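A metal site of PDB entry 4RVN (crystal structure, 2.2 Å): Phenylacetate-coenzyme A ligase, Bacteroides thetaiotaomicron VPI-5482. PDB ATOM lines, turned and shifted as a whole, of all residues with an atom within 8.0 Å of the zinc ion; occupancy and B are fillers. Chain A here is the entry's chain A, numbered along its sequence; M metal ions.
ND1 of His 259 sits at hydrogen-bond distance from O of His 320.
The backbone carbonyl oxygen of Phe 250 lies within hydrogen-bond range of the backbone NH of His 259.
The side-chain sulfur (SG) of Cys 252 sits close to the backbone NH (N) of Glu 254 (3.5 Å).
O of Cys 316 sits at hydrogen-bond distance from OH of Tyr 6, 2.7 Å away.
The guanidinium group (NH1) of Arg 318 lies close to the side-chain sulfur (SG) of Cys 316, at 3.4 Å.
Of the 23 residues printed, 4 come within 4 Å of the zinc ion.
A ring nitrogen (NE2) of His 259 is bound to the zinc ion.
The zinc ion is bound by SG of Cys 316.
The side-chain sulfur (SG) of Cys 252 binds the zinc ion, 2.2 Å away.
SG of Cys 314 binds the zinc ion, at 2.4 Å.
The zinc ion has four donor atoms within binding distance.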
ATOM      1  N   THR A   4       5.415 -28.356  -2.755  1.00  0.00           N
ATOM      2  CA  THR A   4       4.214 -29.099  -2.371  1.00  0.00           C
ATOM      3  C   THR A   4       4.443 -30.610  -2.566  1.00  0.00           C
ATOM      4  O   THR A   4       4.940 -31.040  -3.607  1.00  0.00           O
ATOM      5  CB  THR A   4       2.983 -28.615  -3.180  1.00  0.00           C
ATOM      6  OG1 THR A   4       2.886 -27.188  -3.085  1.00  0.00           O
ATOM      7  CG2 THR A   4       1.675 -29.219  -2.692  1.00  0.00           C
ATOM      8  N   TYR A   6       2.695 -34.553  -2.441  1.00  0.00           N
ATOM      9  CA  TYR A   6       1.432 -35.232  -2.692  1.00  0.00           C
ATOM     10  C   TYR A   6       1.484 -36.718  -2.310  1.00  0.00           C
ATOM     11  O   TYR A   6       2.518 -37.356  -2.446  1.00  0.00           O
ATOM     12  CB  TYR A   6       1.053 -35.117  -4.186  1.00  0.00           C
ATOM     13  CG  TYR A   6       1.190 -33.723  -4.760  1.00  0.00           C
ATOM     14  CD1 TYR A   6       0.146 -32.800  -4.655  1.00  0.00           C
ATOM     15  CD2 TYR A   6       2.337 -33.327  -5.434  1.00  0.00           C
ATOM     16  CE1 TYR A   6       0.267 -31.518  -5.184  1.00  0.00           C
ATOM     17  CE2 TYR A   6       2.468 -32.046  -5.966  1.00  0.00           C
ATOM     18  CZ  TYR A   6       1.433 -31.141  -5.824  1.00  0.00           C
ATOM     19  OH  TYR A   6       1.564 -29.878  -6.349  1.00  0.00           O
ATOM     20  N   MET A 124      -1.910 -34.265   2.667  1.00  0.00           N
ATOM     21  CA  MET A 124      -2.049 -32.969   1.992  1.00  0.00           C
ATOM     22  C   MET A 124      -1.847 -31.796   2.971  1.00  0.00           C
ATOM     23  O   MET A 124      -1.214 -30.798   2.584  1.00  0.00           O
ATOM     24  CB  MET A 124      -3.429 -32.862   1.331  1.00  0.00           C
ATOM     25  CG  MET A 124      -3.717 -31.502   0.702  1.00  0.00           C
ATOM     26  SD  MET A 124      -5.283 -31.453  -0.445  1.00  0.00           S
ATOM     27  CE  MET A 124      -6.617 -31.894   0.823  1.00  0.00           C
ATOM     28  N   PHE A 250     -11.559 -31.649   1.416  1.00  0.00           N
ATOM     29  CA  PHE A 250     -10.619 -31.188   2.442  1.00  0.00           C
ATOM     30  C   PHE A 250      -9.809 -29.999   1.976  1.00  0.00           C
ATOM     31  O   PHE A 250      -9.432 -29.959   0.805  1.00  0.00           O
ATOM     32  CB  PHE A 250      -9.668 -32.372   2.725  1.00  0.00           C
ATOM     33  CG  PHE A 250      -9.252 -32.662   4.138  1.00  0.00           C
ATOM     34  CD1 PHE A 250      -9.973 -33.556   4.924  1.00  0.00           C
ATOM     35  CD2 PHE A 250      -8.054 -32.163   4.639  1.00  0.00           C
ATOM     36  CE1 PHE A 250      -9.521 -33.919   6.186  1.00  0.00           C
ATOM     37  CE2 PHE A 250      -7.616 -32.508   5.921  1.00  0.00           C
ATOM     38  CZ  PHE A 250      -8.353 -33.389   6.685  1.00  0.00           C
ATOM     39  N   GLU A 251      -9.507 -29.050   2.882  1.00  0.00           N
ATOM     40  CA  GLU A 251      -8.657 -27.904   2.563  1.00  0.00           C
ATOM     41  C   GLU A 251      -7.225 -28.324   2.347  1.00  0.00           C
ATOM     42  O   GLU A 251      -6.775 -29.299   2.943  1.00  0.00           O
ATOM     43  CB  GLU A 251      -8.682 -26.848   3.687  1.00  0.00           C
ATOM     44  CG  GLU A 251      -9.896 -25.944   3.751  1.00  0.00           C
ATOM     45  CD  GLU A 251      -9.771 -24.900   4.855  1.00  0.00           C
ATOM     46  OE1 GLU A 251      -9.224 -25.238   5.935  1.00  0.00           O
ATOM     47  OE2 GLU A 251     -10.232 -23.756   4.655  1.00  0.00           O
ATOM     48  N   CYS A 252      -6.495 -27.571   1.519  1.00  0.00           N
ATOM     49  CA  CYS A 252      -5.062 -27.800   1.334  1.00  0.00           C
ATOM     50  C   CYS A 252      -4.328 -26.849   2.293  1.00  0.00           C
ATOM     51  O   CYS A 252      -4.983 -26.247   3.144  1.00  0.00           O
ATOM     52  CB  CYS A 252      -4.643 -27.614  -0.123  1.00  0.00           C
ATOM     53  SG  CYS A 252      -4.908 -25.954  -0.778  1.00  0.00           S
ATOM     54  N   GLN A 253      -3.005 -26.687   2.179  1.00  0.00           N
ATOM     55  CA  GLN A 253      -2.277 -25.813   3.102  1.00  0.00           C
ATOM     56  C   GLN A 253      -2.536 -24.320   2.759  1.00  0.00           C
ATOM     57  O   GLN A 253      -2.168 -23.460   3.554  1.00  0.00           O
ATOM     58  CB  GLN A 253      -0.776 -26.124   3.101  1.00  0.00           C
ATOM     59  CG  GLN A 253      -0.514 -27.489   3.751  1.00  0.00           C
ATOM     60  CD  GLN A 253       0.933 -27.884   3.909  1.00  0.00           C
ATOM     61  OE1 GLN A 253       1.286 -29.062   3.778  1.00  0.00           O
ATOM     62  NE2 GLN A 253       1.807 -26.940   4.229  1.00  0.00           N
ATOM     63  N   GLU A 254      -3.254 -24.033   1.640  1.00  0.00           N
ATOM     64  CA  GLU A 254      -3.640 -22.667   1.249  1.00  0.00           C
ATOM     65  C   GLU A 254      -4.828 -22.173   2.083  1.00  0.00           C
ATOM     66  O   GLU A 254      -5.030 -20.967   2.190  1.00  0.00           O
ATOM     67  CB  GLU A 254      -3.989 -22.573  -0.247  1.00  0.00           C
ATOM     68  CG  GLU A 254      -2.815 -22.828  -1.183  1.00  0.00           C
ATOM     69  CD  GLU A 254      -1.677 -21.826  -1.120  1.00  0.00           C
ATOM     70  OE1 GLU A 254      -1.952 -20.612  -1.015  1.00  0.00           O
ATOM     71  OE2 GLU A 254      -0.504 -22.265  -1.216  1.00  0.00           O
ATOM     72  N   GLN A 255      -5.605 -23.123   2.685  1.00  0.00           N
ATOM     73  CA  GLN A 255      -6.786 -22.870   3.525  1.00  0.00           C
ATOM     74  C   GLN A 255      -7.775 -21.927   2.798  1.00  0.00           C
ATOM     75  O   GLN A 255      -8.246 -20.931   3.362  1.00  0.00           O
ATOM     76  CB  GLN A 255      -6.383 -22.283   4.905  1.00  0.00           C
ATOM     77  CG  GLN A 255      -5.599 -23.242   5.790  1.00  0.00           C
ATOM     78  CD  GLN A 255      -5.165 -22.598   7.085  1.00  0.00           C
ATOM     79  OE1 GLN A 255      -4.636 -21.482   7.108  1.00  0.00           O
ATOM     80  NE2 GLN A 255      -5.327 -23.315   8.177  1.00  0.00           N
ATOM     81  N   ASN A 256      -8.068 -22.252   1.522  1.00  0.00           N
ATOM     82  CA  ASN A 256      -8.971 -21.497   0.670  1.00  0.00           C
ATOM     83  C   ASN A 256      -9.721 -22.471  -0.232  1.00  0.00           C
ATOM     84  O   ASN A 256      -9.278 -22.778  -1.344  1.00  0.00           O
ATOM     85  CB  ASN A 256      -8.213 -20.419  -0.139  1.00  0.00           C
ATOM     86  CG  ASN A 256      -9.088 -19.559  -1.027  1.00  0.00           C
ATOM     87  OD1 ASN A 256      -8.665 -19.152  -2.122  1.00  0.00           O
ATOM     88  ND2 ASN A 256     -10.326 -19.275  -0.611  1.00  0.00           N
ATOM     89  N   GLY A 257     -10.844 -22.961   0.291  1.00  0.00           N
ATOM     90  CA  GLY A 257     -11.679 -23.937  -0.396  1.00  0.00           C
ATOM     91  C   GLY A 257     -11.247 -25.353  -0.123  1.00  0.00           C
ATOM     92  O   GLY A 257     -10.051 -25.614   0.108  1.00  0.00           O
ATOM     93  N   MET A 258     -12.214 -26.285  -0.154  1.00  0.00           N
ATOM     94  CA  MET A 258     -11.956 -27.695   0.092  1.00  0.00           C
ATOM     95  C   MET A 258     -11.871 -28.465  -1.218  1.00  0.00           C
ATOM     96  O   MET A 258     -12.860 -28.523  -1.964  1.00  0.00           O
ATOM     97  CB  MET A 258     -13.049 -28.295   1.000  1.00  0.00           C
ATOM     98  CG  MET A 258     -12.980 -27.784   2.433  1.00  0.00           C
ATOM     99  SD  MET A 258     -14.358 -28.524   3.545  1.00  0.00           S
ATOM    100  CE  MET A 258     -15.914 -27.619   2.852  1.00  0.00           C
ATOM    101  N   HIS A 259     -10.700 -29.055  -1.503  1.00  0.00           N
ATOM    102  CA  HIS A 259     -10.471 -29.875  -2.697  1.00  0.00           C
ATOM    103  C   HIS A 259     -11.322 -31.144  -2.644  1.00  0.00           C
ATOM    104  O   HIS A 259     -11.192 -31.940  -1.714  1.00  0.00           O
ATOM    105  CB  HIS A 259      -8.994 -30.268  -2.871  1.00  0.00           C
ATOM    106  CG  HIS A 259      -8.088 -29.139  -3.245  1.00  0.00           C
ATOM    107  ND1 HIS A 259      -7.950 -28.747  -4.568  1.00  0.00           N
ATOM    108  CD2 HIS A 259      -7.258 -28.403  -2.483  1.00  0.00           C
ATOM    109  CE1 HIS A 259      -7.067 -27.759  -4.553  1.00  0.00           C
ATOM    110  NE2 HIS A 259      -6.615 -27.517  -3.319  1.00  0.00           N
ATOM    111  N   TRP A 261     -12.238 -34.771  -4.128  1.00  0.00           N
ATOM    112  CA  TRP A 261     -11.502 -35.785  -4.890  1.00  0.00           C
ATOM    113  C   TRP A 261     -12.404 -36.333  -5.986  1.00  0.00           C
ATOM    114  O   TRP A 261     -13.207 -37.240  -5.777  1.00  0.00           O
ATOM    115  CB  TRP A 261     -10.947 -36.888  -3.971  1.00  0.00           C
ATOM    116  CG  TRP A 261     -10.008 -36.347  -2.929  1.00  0.00           C
ATOM    117  CD1 TRP A 261     -10.197 -36.372  -1.578  1.00  0.00           C
ATOM    118  CD2 TRP A 261      -8.823 -35.571  -3.153  1.00  0.00           C
ATOM    119  NE1 TRP A 261      -9.150 -35.736  -0.946  1.00  0.00           N
ATOM    120  CE2 TRP A 261      -8.303 -35.212  -1.894  1.00  0.00           C
ATOM    121  CE3 TRP A 261      -8.126 -35.156  -4.314  1.00  0.00           C
ATOM    122  CZ2 TRP A 261      -7.115 -34.473  -1.740  1.00  0.00           C
ATOM    123  CZ3 TRP A 261      -6.961 -34.410  -4.167  1.00  0.00           C
ATOM    124  CH2 TRP A 261      -6.459 -34.088  -2.889  1.00  0.00           C
ATOM    125  N   LYS A 313      -7.476 -21.690 -10.522  1.00  0.00           N
ATOM    126  CA  LYS A 313      -6.499 -22.715 -10.149  1.00  0.00           C
ATOM    127  C   LYS A 313      -5.994 -22.481  -8.730  1.00  0.00           C
ATOM    128  O   LYS A 313      -5.847 -21.314  -8.340  1.00  0.00           O
ATOM    129  CB  LYS A 313      -5.310 -22.699 -11.131  1.00  0.00           C
ATOM    130  CG  LYS A 313      -5.651 -22.963 -12.591  1.00  0.00           C
ATOM    131  CD  LYS A 313      -4.390 -22.929 -13.436  1.00  0.00           C
ATOM    132  CE  LYS A 313      -4.658 -23.200 -14.893  1.00  0.00           C
ATOM    133  NZ  LYS A 313      -3.405 -23.171 -15.691  1.00  0.00           N
ATOM    134  N   CYS A 314      -5.693 -23.544  -7.978  1.00  0.00           N
ATOM    135  CA  CYS A 314      -5.161 -23.387  -6.629  1.00  0.00           C
ATOM    136  C   CYS A 314      -3.619 -23.362  -6.673  1.00  0.00           C
ATOM    137  O   CYS A 314      -3.041 -24.200  -7.371  1.00  0.00           O
ATOM    138  CB  CYS A 314      -5.672 -24.473  -5.684  1.00  0.00           C
ATOM    139  SG  CYS A 314      -5.162 -24.238  -3.957  1.00  0.00           S
ATOM    140  N   PRO A 315      -2.951 -22.476  -5.891  1.00  0.00           N
ATOM    141  CA  PRO A 315      -1.473 -22.434  -5.911  1.00  0.00           C
ATOM    142  C   PRO A 315      -0.787 -23.717  -5.400  1.00  0.00           C
ATOM    143  O   PRO A 315       0.432 -23.829  -5.594  1.00  0.00           O
ATOM    144  CB  PRO A 315      -1.147 -21.270  -4.968  1.00  0.00           C
ATOM    145  CG  PRO A 315      -2.363 -20.431  -4.968  1.00  0.00           C
ATOM    146  CD  PRO A 315      -3.489 -21.402  -5.035  1.00  0.00           C
ATOM    147  N   CYS A 316      -1.522 -24.684  -4.793  1.00  0.00           N
ATOM    148  CA  CYS A 316      -0.916 -25.928  -4.315  1.00  0.00           C
ATOM    149  C   CYS A 316      -0.624 -26.866  -5.519  1.00  0.00           C
ATOM    150  O   CYS A 316       0.075 -27.867  -5.356  1.00  0.00           O
ATOM    151  CB  CYS A 316      -1.778 -26.621  -3.269  1.00  0.00           C
ATOM    152  SG  CYS A 316      -3.266 -27.433  -3.912  1.00  0.00           S
ATOM    153  N   GLY A 317      -1.159 -26.532  -6.701  1.00  0.00           N
ATOM    154  CA  GLY A 317      -0.957 -27.291  -7.930  1.00  0.00           C
ATOM    155  C   GLY A 317      -1.985 -28.365  -8.213  1.00  0.00           C
ATOM    156  O   GLY A 317      -1.981 -28.944  -9.301  1.00  0.00           O
ATOM    157  N   ARG A 318      -2.872 -28.640  -7.242  1.00  0.00           N
ATOM    158  CA  ARG A 318      -3.914 -29.663  -7.405  1.00  0.00           C
ATOM    159  C   ARG A 318      -5.008 -29.139  -8.326  1.00  0.00           C
ATOM    160  O   ARG A 318      -5.433 -27.974  -8.224  1.00  0.00           O
ATOM    161  CB  ARG A 318      -4.487 -30.114  -6.060  1.00  0.00           C
ATOM    162  CG  ARG A 318      -3.465 -30.892  -5.224  1.00  0.00           C
ATOM    163  CD  ARG A 318      -3.966 -31.202  -3.841  1.00  0.00           C
ATOM    164  NE  ARG A 318      -2.979 -31.947  -3.062  1.00  0.00           N
ATOM    165  CZ  ARG A 318      -2.044 -31.394  -2.289  1.00  0.00           C
ATOM    166  NH1 ARG A 318      -1.975 -30.071  -2.175  1.00  0.00           N
ATOM    167  NH2 ARG A 318      -1.193 -32.150  -1.618  1.00  0.00           N
ATOM    168  N   THR A 319      -5.427 -29.997  -9.262  1.00  0.00           N
ATOM    169  CA  THR A 319      -6.409 -29.718 -10.318  1.00  0.00           C
ATOM    170  C   THR A 319      -7.845 -30.075  -9.900  1.00  0.00           C
ATOM    171  O   THR A 319      -8.786 -29.708 -10.614  1.00  0.00           O
ATOM    172  CB  THR A 319      -6.027 -30.520 -11.566  1.00  0.00           C
ATOM    173  OG1 THR A 319      -5.922 -31.905 -11.203  1.00  0.00           O
ATOM    174  CG2 THR A 319      -4.717 -30.040 -12.199  1.00  0.00           C
ATOM    175  N   HIS A 320      -8.018 -30.781  -8.776  1.00  0.00           N
ATOM    176  CA  HIS A 320      -9.320 -31.160  -8.248  1.00  0.00           C
ATOM    177  C   HIS A 320     -10.050 -29.916  -7.736  1.00  0.00           C
ATOM    178  O   HIS A 320      -9.456 -29.142  -6.969  1.00  0.00           O
ATOM    179  CB  HIS A 320      -9.158 -32.222  -7.144  1.00  0.00           C
ATOM    180  CG  HIS A 320      -8.676 -33.541  -7.663  1.00  0.00           C
ATOM    181  ND1 HIS A 320      -9.539 -34.597  -7.848  1.00  0.00           N
ATOM    182  CD2 HIS A 320      -7.438 -33.903  -8.061  1.00  0.00           C
ATOM    183  CE1 HIS A 320      -8.802 -35.585  -8.321  1.00  0.00           C
ATOM    184  NE2 HIS A 320      -7.528 -35.214  -8.472  1.00  0.00           N
ATOM    185  N   ARG A 322     -12.438 -27.020  -5.973  1.00  0.00           N
ATOM    186  CA  ARG A 322     -12.596 -26.577  -4.589  1.00  0.00           C
ATOM    187  C   ARG A 322     -14.000 -26.088  -4.328  1.00  0.00           C
ATOM    188  O   ARG A 322     -14.553 -25.324  -5.127  1.00  0.00           O
ATOM    189  CB  ARG A 322     -11.590 -25.462  -4.248  1.00  0.00           C
ATOM    190  CG  ARG A 322     -10.129 -25.909  -4.209  1.00  0.00           C
ATOM    191  CD  ARG A 322      -9.150 -24.736  -4.158  1.00  0.00           C
ATOM    192  NE  ARG A 322      -9.238 -23.883  -5.353  1.00  0.00           N
ATOM    193  CZ  ARG A 322      -9.779 -22.669  -5.376  1.00  0.00           C
ATOM    194  NH1 ARG A 322     -10.235 -22.117  -4.259  1.00  0.00           N
ATOM    195  NH2 ARG A 322      -9.826 -21.982  -6.503  1.00  0.00           N
HETATM  196 ZN    ZN M   1      -5.015 -26.453  -2.967  1.00  0.00          ZN
